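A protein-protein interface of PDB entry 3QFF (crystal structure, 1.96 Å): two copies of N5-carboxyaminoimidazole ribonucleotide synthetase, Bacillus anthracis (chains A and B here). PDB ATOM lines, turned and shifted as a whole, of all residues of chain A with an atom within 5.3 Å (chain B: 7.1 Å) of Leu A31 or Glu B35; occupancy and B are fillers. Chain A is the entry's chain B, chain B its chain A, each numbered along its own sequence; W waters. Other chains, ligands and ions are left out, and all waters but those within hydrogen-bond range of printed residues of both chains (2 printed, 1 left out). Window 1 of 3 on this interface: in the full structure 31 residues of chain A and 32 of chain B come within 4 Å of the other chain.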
ATOM      1  N   GLY A  26     -13.304 -10.383   2.419  1.00  0.00           N
ATOM      2  CA  GLY A  26     -12.943 -11.056   1.157  1.00  0.00           C
ATOM      3  C   GLY A  26     -11.542 -10.678   0.688  1.00  0.00           C
ATOM      4  O   GLY A  26     -10.795 -11.533   0.225  1.00  0.00           O
ATOM      5  N   ARG A  27     -11.179  -9.407   0.831  1.00  0.00           N
ATOM      6  CA  ARG A  27      -9.827  -8.941   0.504  1.00  0.00           C
ATOM      7  C   ARG A  27      -8.759  -9.721   1.279  1.00  0.00           C
ATOM      8  O   ARG A  27      -7.772 -10.184   0.705  1.00  0.00           O
ATOM      9  CB  ARG A  27      -9.681  -7.431   0.761  1.00  0.00           C
ATOM     10  CG  ARG A  27      -8.260  -6.853   0.484  1.00  0.00           C
ATOM     11  CD  ARG A  27      -8.110  -5.451   1.079  1.00  0.00           C
ATOM     12  NE  ARG A  27      -6.796  -4.828   0.857  1.00  0.00           N
ATOM     13  CZ  ARG A  27      -6.460  -4.138  -0.232  1.00  0.00           C
ATOM     14  NH1 ARG A  27      -7.329  -4.006  -1.231  1.00  0.00           N
ATOM     15  NH2 ARG A  27      -5.248  -3.589  -0.337  1.00  0.00           N
ATOM     16  N   MET A  28      -8.956  -9.872   2.584  1.00  0.00           N
ATOM     17  CA  MET A  28      -7.976 -10.574   3.404  1.00  0.00           C
ATOM     18  C   MET A  28      -7.970 -12.085   3.150  1.00  0.00           C
ATOM     19  O   MET A  28      -6.909 -12.718   3.199  1.00  0.00           O
ATOM     20  CB  MET A  28      -8.163 -10.218   4.886  1.00  0.00           C
ATOM     21  CG  MET A  28      -7.695  -8.778   5.174  1.00  0.00           C
ATOM     22  SD  MET A  28      -7.892  -8.212   6.870  1.00  0.00           S
ATOM     23  CE  MET A  28      -9.641  -7.833   6.940  1.00  0.00           C
ATOM     24  N   MET A  29      -9.146 -12.656   2.884  1.00  0.00           N
ATOM     25  CA  MET A  29      -9.234 -14.043   2.388  1.00  0.00           C
ATOM     26  C   MET A  29      -8.386 -14.197   1.137  1.00  0.00           C
ATOM     27  O   MET A  29      -7.569 -15.108   1.046  1.00  0.00           O
ATOM     28  CB  MET A  29     -10.678 -14.402   2.015  1.00  0.00           C
ATOM     29  CG  MET A  29     -11.578 -14.747   3.194  1.00  0.00           C
ATOM     30  SD  MET A  29     -13.237 -15.121   2.567  1.00  0.00           S
ATOM     31  CE  MET A  29     -14.200 -15.052   4.073  1.00  0.00           C
ATOM     32  N   ALA A  30      -8.606 -13.288   0.184  1.00  0.00           N
ATOM     33  CA  ALA A  30      -7.920 -13.292  -1.111  1.00  0.00           C
ATOM     34  C   ALA A  30      -6.400 -13.198  -0.953  1.00  0.00           C
ATOM     35  O   ALA A  30      -5.680 -13.972  -1.567  1.00  0.00           O
ATOM     36  CB  ALA A  30      -8.443 -12.180  -1.998  1.00  0.00           C
ATOM     37  N   LEU A  31      -5.917 -12.283  -0.110  1.00  0.00           N
ATOM     38  CA  LEU A  31      -4.466 -12.168   0.112  1.00  0.00           C
ATOM     39  C   LEU A  31      -3.849 -13.472   0.636  1.00  0.00           C
ATOM     40  O   LEU A  31      -2.793 -13.896   0.161  1.00  0.00           O
ATOM     41  CB  LEU A  31      -4.125 -10.987   1.045  1.00  0.00           C
ATOM     42  CG  LEU A  31      -4.439  -9.618   0.434  1.00  0.00           C
ATOM     43  CD1 LEU A  31      -4.537  -8.534   1.483  1.00  0.00           C
ATOM     44  CD2 LEU A  31      -3.427  -9.246  -0.668  1.00  0.00           C
ATOM     45  N   ALA A  32      -4.509 -14.099   1.608  1.00  0.00           N
ATOM     46  CA  ALA A  32      -4.052 -15.365   2.189  1.00  0.00           C
ATOM     47  C   ALA A  32      -4.097 -16.519   1.185  1.00  0.00           C
ATOM     48  O   ALA A  32      -3.207 -17.370   1.175  1.00  0.00           O
ATOM     49  CB  ALA A  32      -4.874 -15.706   3.427  1.00  0.00           C
ATOM     50  N   ALA A  33      -5.143 -16.559   0.362  1.00  0.00           N
ATOM     51  CA  ALA A  33      -5.235 -17.562  -0.700  1.00  0.00           C
ATOM     52  C   ALA A  33      -4.146 -17.379  -1.762  1.00  0.00           C
ATOM     53  O   ALA A  33      -3.604 -18.357  -2.284  1.00  0.00           O
ATOM     54  CB  ALA A  33      -6.609 -17.522  -1.346  1.00  0.00           C
ATOM     55  N   LYS A  34      -3.831 -16.124  -2.078  1.00  0.00           N
ATOM     56  CA  LYS A  34      -2.775 -15.829  -3.053  1.00  0.00           C
ATOM     57  C   LYS A  34      -1.412 -16.340  -2.614  1.00  0.00           C
ATOM     58  O   LYS A  34      -0.636 -16.832  -3.439  1.00  0.00           O
ATOM     59  CB  LYS A  34      -2.689 -14.332  -3.330  1.00  0.00           C
ATOM     60  CG  LYS A  34      -3.825 -13.809  -4.183  1.00  0.00           C
ATOM     61  CD  LYS A  34      -3.432 -13.811  -5.627  1.00  0.00           C
ATOM     62  CE  LYS A  34      -4.406 -12.994  -6.452  1.00  0.00           C
ATOM     63  NZ  LYS A  34      -4.195 -13.328  -7.882  1.00  0.00           N
ATOM     64  N   GLU A  35      -1.109 -16.237  -1.326  1.00  0.00           N
ATOM     65  CA  GLU A  35       0.170 -16.747  -0.856  1.00  0.00           C
ATOM     66  C   GLU A  35       0.312 -18.243  -1.123  1.00  0.00           C
ATOM     67  O   GLU A  35       1.397 -18.700  -1.436  1.00  0.00           O
ATOM     68  CB  GLU A  35       0.464 -16.370   0.607  1.00  0.00           C
ATOM     69  CG  GLU A  35       1.354 -15.111   0.725  1.00  0.00           C
ATOM     70  CD  GLU A  35       2.871 -15.397   0.768  1.00  0.00           C
ATOM     71  OE1 GLU A  35       3.409 -15.380   1.905  1.00  0.00           O
ATOM     72  OE2 GLU A  35       3.544 -15.610  -0.279  1.00  0.00           O
ATOM     73  N   VAL A  54      -7.476  -7.192  -5.291  1.00  0.00           N
ATOM     74  CA  VAL A  54      -6.581  -8.333  -5.075  1.00  0.00           C
ATOM     75  C   VAL A  54      -6.936  -9.540  -5.962  1.00  0.00           C
ATOM     76  O   VAL A  54      -6.156 -10.494  -6.081  1.00  0.00           O
ATOM     77  CB  VAL A  54      -6.564  -8.720  -3.556  1.00  0.00           C
ATOM     78  CG1 VAL A  54      -5.801 -10.020  -3.305  1.00  0.00           C
ATOM     79  CG2 VAL A  54      -5.965  -7.568  -2.720  1.00  0.00           C
ATOM     80  N   LEU A 341       0.084  -2.295  10.605  1.00  0.00           N
ATOM     81  CA  LEU A 341      -1.008  -1.576   9.958  1.00  0.00           C
ATOM     82  C   LEU A 341      -1.607  -2.345   8.783  1.00  0.00           C
ATOM     83  O   LEU A 341      -0.884  -2.895   7.954  1.00  0.00           O
ATOM     84  CB  LEU A 341      -0.479  -0.223   9.485  1.00  0.00           C
ATOM     85  CG  LEU A 341      -1.387   0.744   8.744  1.00  0.00           C
ATOM     86  CD1 LEU A 341      -2.588   1.159   9.596  1.00  0.00           C
ATOM     87  CD2 LEU A 341      -0.545   1.954   8.361  1.00  0.00           C
ATOM     88  N   HIS A 342      -2.932  -2.392   8.735  1.00  0.00           N
ATOM     89  CA  HIS A 342      -3.654  -3.050   7.666  1.00  0.00           C
ATOM     90  C   HIS A 342      -4.694  -2.054   7.211  1.00  0.00           C
ATOM     91  O   HIS A 342      -5.494  -1.582   8.023  1.00  0.00           O
ATOM     92  CB  HIS A 342      -4.346  -4.332   8.159  1.00  0.00           C
ATOM     93  CG  HIS A 342      -3.396  -5.392   8.627  1.00  0.00           C
ATOM     94  ND1 HIS A 342      -3.079  -6.494   7.863  1.00  0.00           N
ATOM     95  CD2 HIS A 342      -2.694  -5.517   9.781  1.00  0.00           C
ATOM     96  CE1 HIS A 342      -2.217  -7.251   8.522  1.00  0.00           C
ATOM     97  NE2 HIS A 342      -1.965  -6.681   9.687  1.00  0.00           N
ATOM     98  N   LEU A 343      -4.656  -1.699   5.933  1.00  0.00           N
ATOM     99  CA  LEU A 343      -5.649  -0.789   5.376  1.00  0.00           C
ATOM    100  C   LEU A 343      -6.304  -1.422   4.168  1.00  0.00           C
ATOM    101  O   LEU A 343      -5.626  -2.026   3.344  1.00  0.00           O
ATOM    102  CB  LEU A 343      -5.035   0.570   5.041  1.00  0.00           C
ATOM    103  CG  LEU A 343      -4.538   1.379   6.245  1.00  0.00           C
ATOM    104  CD1 LEU A 343      -3.604   2.475   5.755  1.00  0.00           C
ATOM    105  CD2 LEU A 343      -5.706   1.991   7.035  1.00  0.00           C
ATOM    106  N   ARG B  27       6.189 -10.589  -6.357  1.00  0.00           N
ATOM    107  CA  ARG B  27       4.862 -10.988  -5.878  1.00  0.00           C
ATOM    108  C   ARG B  27       4.749 -10.863  -4.353  1.00  0.00           C
ATOM    109  O   ARG B  27       3.771 -10.326  -3.833  1.00  0.00           O
ATOM    110  CB  ARG B  27       4.561 -12.424  -6.310  1.00  0.00           C
ATOM    111  CG  ARG B  27       3.244 -13.008  -5.766  1.00  0.00           C
ATOM    112  CD  ARG B  27       3.212 -14.494  -6.110  1.00  0.00           C
ATOM    113  NE  ARG B  27       1.990 -15.197  -5.709  1.00  0.00           N
ATOM    114  CZ  ARG B  27       0.915 -15.360  -6.482  1.00  0.00           C
ATOM    115  NH1 ARG B  27       0.866 -14.821  -7.694  1.00  0.00           N
ATOM    116  NH2 ARG B  27      -0.131 -16.052  -6.026  1.00  0.00           N
ATOM    117  N   MET B  28       5.758 -11.352  -3.648  1.00  0.00           N
ATOM    118  CA  MET B  28       5.738 -11.296  -2.188  1.00  0.00           C
ATOM    119  C   MET B  28       5.878  -9.877  -1.610  1.00  0.00           C
ATOM    120  O   MET B  28       5.239  -9.560  -0.598  1.00  0.00           O
ATOM    121  CB  MET B  28       6.754 -12.269  -1.602  1.00  0.00           C
ATOM    122  CG  MET B  28       6.264 -13.709  -1.719  1.00  0.00           C
ATOM    123  SD  MET B  28       7.426 -14.934  -1.120  1.00  0.00           S
ATOM    124  CE  MET B  28       8.691 -14.971  -2.397  1.00  0.00           C
ATOM    125  N   MET B  29       6.663  -9.021  -2.262  1.00  0.00           N
ATOM    126  CA  MET B  29       6.713  -7.587  -1.885  1.00  0.00           C
ATOM    127  C   MET B  29       5.305  -7.004  -2.059  1.00  0.00           C
ATOM    128  O   MET B  29       4.808  -6.234  -1.228  1.00  0.00           O
ATOM    129  CB  MET B  29       7.649  -6.802  -2.828  1.00  0.00           C
ATOM    130  CG  MET B  29       9.159  -6.908  -2.586  1.00  0.00           C
ATOM    131  SD  MET B  29      10.027  -5.907  -3.858  1.00  0.00           S
ATOM    132  CE  MET B  29      11.744  -6.355  -3.591  1.00  0.00           C
ATOM    133  N   ALA B  30       4.688  -7.353  -3.181  1.00  0.00           N
ATOM    134  CA  ALA B  30       3.407  -6.770  -3.569  1.00  0.00           C
ATOM    135  C   ALA B  30       2.274  -7.213  -2.644  1.00  0.00           C
ATOM    136  O   ALA B  30       1.383  -6.420  -2.327  1.00  0.00           O
ATOM    137  CB  ALA B  30       3.095  -7.106  -5.026  1.00  0.00           C
ATOM    138  N   LEU B  31       2.320  -8.471  -2.203  1.00  0.00           N
ATOM    139  CA  LEU B  31       1.352  -8.979  -1.218  1.00  0.00           C
ATOM    140  C   LEU B  31       1.466  -8.261   0.125  1.00  0.00           C
ATOM    141  O   LEU B  31       0.452  -7.910   0.740  1.00  0.00           O
ATOM    142  CB  LEU B  31       1.479 -10.500  -1.050  1.00  0.00           C
ATOM    143  CG  LEU B  31       0.901 -11.296  -2.249  1.00  0.00           C
ATOM    144  CD1 LEU B  31       1.403 -12.726  -2.258  1.00  0.00           C
ATOM    145  CD2 LEU B  31      -0.628 -11.288  -2.224  1.00  0.00           C
ATOM    146  N   ALA B  32       2.704  -8.014   0.551  1.00  0.00           N
ATOM    147  CA  ALA B  32       2.987  -7.275   1.786  1.00  0.00           C
ATOM    148  C   ALA B  32       2.478  -5.836   1.672  1.00  0.00           C
ATOM    149  O   ALA B  32       1.902  -5.277   2.618  1.00  0.00           O
ATOM    150  CB  ALA B  32       4.517  -7.280   2.049  1.00  0.00           C
ATOM    151  N   ALA B  33       2.709  -5.226   0.509  1.00  0.00           N
ATOM    152  CA  ALA B  33       2.343  -3.819   0.302  1.00  0.00           C
ATOM    153  C   ALA B  33       0.821  -3.654   0.288  1.00  0.00           C
ATOM    154  O   ALA B  33       0.289  -2.656   0.766  1.00  0.00           O
ATOM    155  CB  ALA B  33       2.946  -3.308  -1.001  1.00  0.00           C
ATOM    156  N   LYS B  34       0.142  -4.648  -0.279  1.00  0.00           N
ATOM    157  CA  LYS B  34      -1.313  -4.639  -0.414  1.00  0.00           C
ATOM    158  C   LYS B  34      -1.996  -4.684   0.965  1.00  0.00           C
ATOM    159  O   LYS B  34      -3.026  -4.044   1.164  1.00  0.00           O
ATOM    160  CB  LYS B  34      -1.750  -5.810  -1.294  1.00  0.00           C
ATOM    161  CG  LYS B  34      -2.672  -5.435  -2.455  1.00  0.00           C
ATOM    162  CD  LYS B  34      -1.894  -4.943  -3.656  1.00  0.00           C
ATOM    163  CE  LYS B  34      -2.766  -4.928  -4.912  1.00  0.00           C
ATOM    164  NZ  LYS B  34      -3.673  -3.745  -4.968  1.00  0.00           N
ATOM    165  N   GLU B  35      -1.415  -5.419   1.922  1.00  0.00           N
ATOM    166  CA  GLU B  35      -1.978  -5.479   3.289  1.00  0.00           C
ATOM    167  C   GLU B  35      -2.035  -4.093   3.919  1.00  0.00           C
ATOM    168  O   GLU B  35      -2.955  -3.786   4.671  1.00  0.00           O
ATOM    169  CB  GLU B  35      -1.191  -6.446   4.186  1.00  0.00           C
ATOM    170  CG  GLU B  35      -1.468  -7.911   3.833  1.00  0.00           C
ATOM    171  CD  GLU B  35      -0.392  -8.879   4.281  1.00  0.00           C
ATOM    172  OE1 GLU B  35       0.218  -8.661   5.361  1.00  0.00           O
ATOM    173  OE2 GLU B  35      -0.178  -9.889   3.550  1.00  0.00           O
ATOM    174  N   MET B  36      -1.057  -3.264   3.569  1.00  0.00           N
ATOM    175  CA  MET B  36      -0.921  -1.913   4.085  1.00  0.00           C
ATOM    176  C   MET B  36      -1.610  -0.884   3.196  1.00  0.00           C
ATOM    177  O   MET B  36      -1.480   0.310   3.424  1.00  0.00           O
ATOM    178  CB  MET B  36       0.566  -1.563   4.246  1.00  0.00           C
ATOM    179  CG  MET B  36       1.150  -1.957   5.603  1.00  0.00           C
ATOM    180  SD  MET B  36       2.896  -1.494   5.805  1.00  0.00           S
ATOM    181  CE  MET B  36       3.639  -2.557   4.585  1.00  0.00           C
ATOM    182  N   GLY B  37      -2.324  -1.356   2.178  1.00  0.00           N
ATOM    183  CA  GLY B  37      -3.166  -0.507   1.351  1.00  0.00           C
ATOM    184  C   GLY B  37      -2.442   0.241   0.249  1.00  0.00           C
ATOM    185  O   GLY B  37      -2.930   1.274  -0.203  1.00  0.00           O
ATOM    186  N   TYR B  38      -1.274  -0.258  -0.166  1.00  0.00           N
ATOM    187  CA  TYR B  38      -0.582   0.277  -1.340  1.00  0.00           C
ATOM    188  C   TYR B  38      -1.132  -0.310  -2.637  1.00  0.00           C
ATOM    189  O   TYR B  38      -1.632  -1.440  -2.670  1.00  0.00           O
ATOM    190  CB  TYR B  38       0.935   0.033  -1.259  1.00  0.00           C
ATOM    191  CG  TYR B  38       1.593   0.867  -0.207  1.00  0.00           C
ATOM    192  CD1 TYR B  38       1.940   2.194  -0.458  1.00  0.00           C
ATOM    193  CD2 TYR B  38       1.838   0.344   1.068  1.00  0.00           C
ATOM    194  CE1 TYR B  38       2.528   2.977   0.517  1.00  0.00           C
ATOM    195  CE2 TYR B  38       2.429   1.127   2.062  1.00  0.00           C
ATOM    196  CZ  TYR B  38       2.773   2.436   1.781  1.00  0.00           C
ATOM    197  OH  TYR B  38       3.355   3.199   2.768  1.00  0.00           O
ATOM    198  N   VAL B  54      -0.866 -10.117  -8.802  1.00  0.00           N
ATOM    199  CA  VAL B  54      -1.284  -9.357  -7.636  1.00  0.00           C
ATOM    200  C   VAL B  54      -1.199  -7.848  -7.885  1.00  0.00           C
ATOM    201  O   VAL B  54      -1.525  -7.068  -7.013  1.00  0.00           O
ATOM    202  CB  VAL B  54      -0.510  -9.778  -6.335  1.00  0.00           C
ATOM    203  CG1 VAL B  54      -0.668 -11.271  -6.064  1.00  0.00           C
ATOM    204  CG2 VAL B  54       0.952  -9.450  -6.429  1.00  0.00           C
HETATM  205  O   HOH W   1       2.846 -16.528  -3.411  1.00  0.00           O
HETATM  206  O   HOH W   2      -4.202  -1.840  -2.545  1.00  0.00           O
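Arg A27 touches Lys B34, and with the chains exchanged Lys A34 touches Arg B27. Leu A31 touches its own counterpart, Leu B31. Leu A31 touches Lys B34, and with the chains exchanged Lys A34 touches Leu B31. Lys A34 touches Val B54, and with the chains exchanged Val A54 touches Lys B34.
Of the 13 printed residues of chain B, 8 touch a printed residue of chain A. Hydrophobic or aromatic side chains of chain B within 4 Å of the printed part of chain A: Met B28, Leu B31, Met B36 and Val B54. Along chain B the printed residues that touch a printed residue of chain A span positions 27 to 54. Of the 14 printed residues of chain A, 8 touch a printed residue of chain B. Hydrophobic or aromatic side chains of chain A that line the printed part of chain B: Leu A31, Val A54, His A342 and Leu A343.
The backbone carbonyl oxygen (O) of Lys A34 sits at hydrogen-bond distance from the guanidinium group (NH2) of Arg B27, at 2.7 Å. NH2 of Arg A27 is in hydrogen-bond range of O of Lys B34 (2.7 Å). O of Glu B35 sits at hydrogen-bond distance from N of Leu A343 (3.0 Å).
Printed residues of chain A within 4 Å of Glu B35: Leu A31 (3.9 Å), Leu A341 (3.98 Å), His A342 (3.2 Å) and Leu A343 (3.0 Å). Printed residues of chain B within 4 Å of Leu A343: Lys B34, Glu B35, Met B36 and Gly B37. Printed residues of chain B within 4 Å of His A342: Glu B35 (3.2 Å). Of the printed residues of chain A, Met B36 touches Leu A341 and Leu A343. Printed residues of chain A within 4 Å of Gly B37: Leu A343 (3.5 Å). Met A28 touches none of the printed residues of chain B. Gly A26 touches none of the printed residues of chain B. The nearest residue of chain B that does not touch Leu A31 is Ala B30 (5.8 Å). The nearest printed residue of chain B that does not touch Leu A343 is Tyr B38 (5.9 Å).
Water W2 lies within hydrogen-bond range of the backbone carbonyl oxygen (O) of Tyr B38 (2.6 Å), the guanidinium group (NH2) of Arg A27 (3.0 Å) and the side-chain amino group (NZ) of Lys B34 (3.1 Å). Water W1 lies within hydrogen-bond range of the guanidinium group of Arg B27 (2.8 Å), the backbone carbonyl oxygen of Glu A35 (3.3 Å) and the backbone carbonyl oxygen of Lys A34 (3.5 Å).
Leu B31 touches Leu A31 (CD2 to CD2, 3.8 Å). CD2 of Leu A31 touches CB of Lys B34, at 3.9 Å. Glu B35 touches Leu A31. Val B54 touches Lys A34. Met B28 touches Glu A35 (CG to OE2, 3.6 Å). Glu A35 touches Leu B31. Leu A341 touches Met B36 (O to CG, 3.2 Å). Glu B35 touches His A342. O of Leu A343 touches O of Lys B34, 3.9 Å away. O of Leu A343 touches CA of Gly B37 (3.5 Å).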
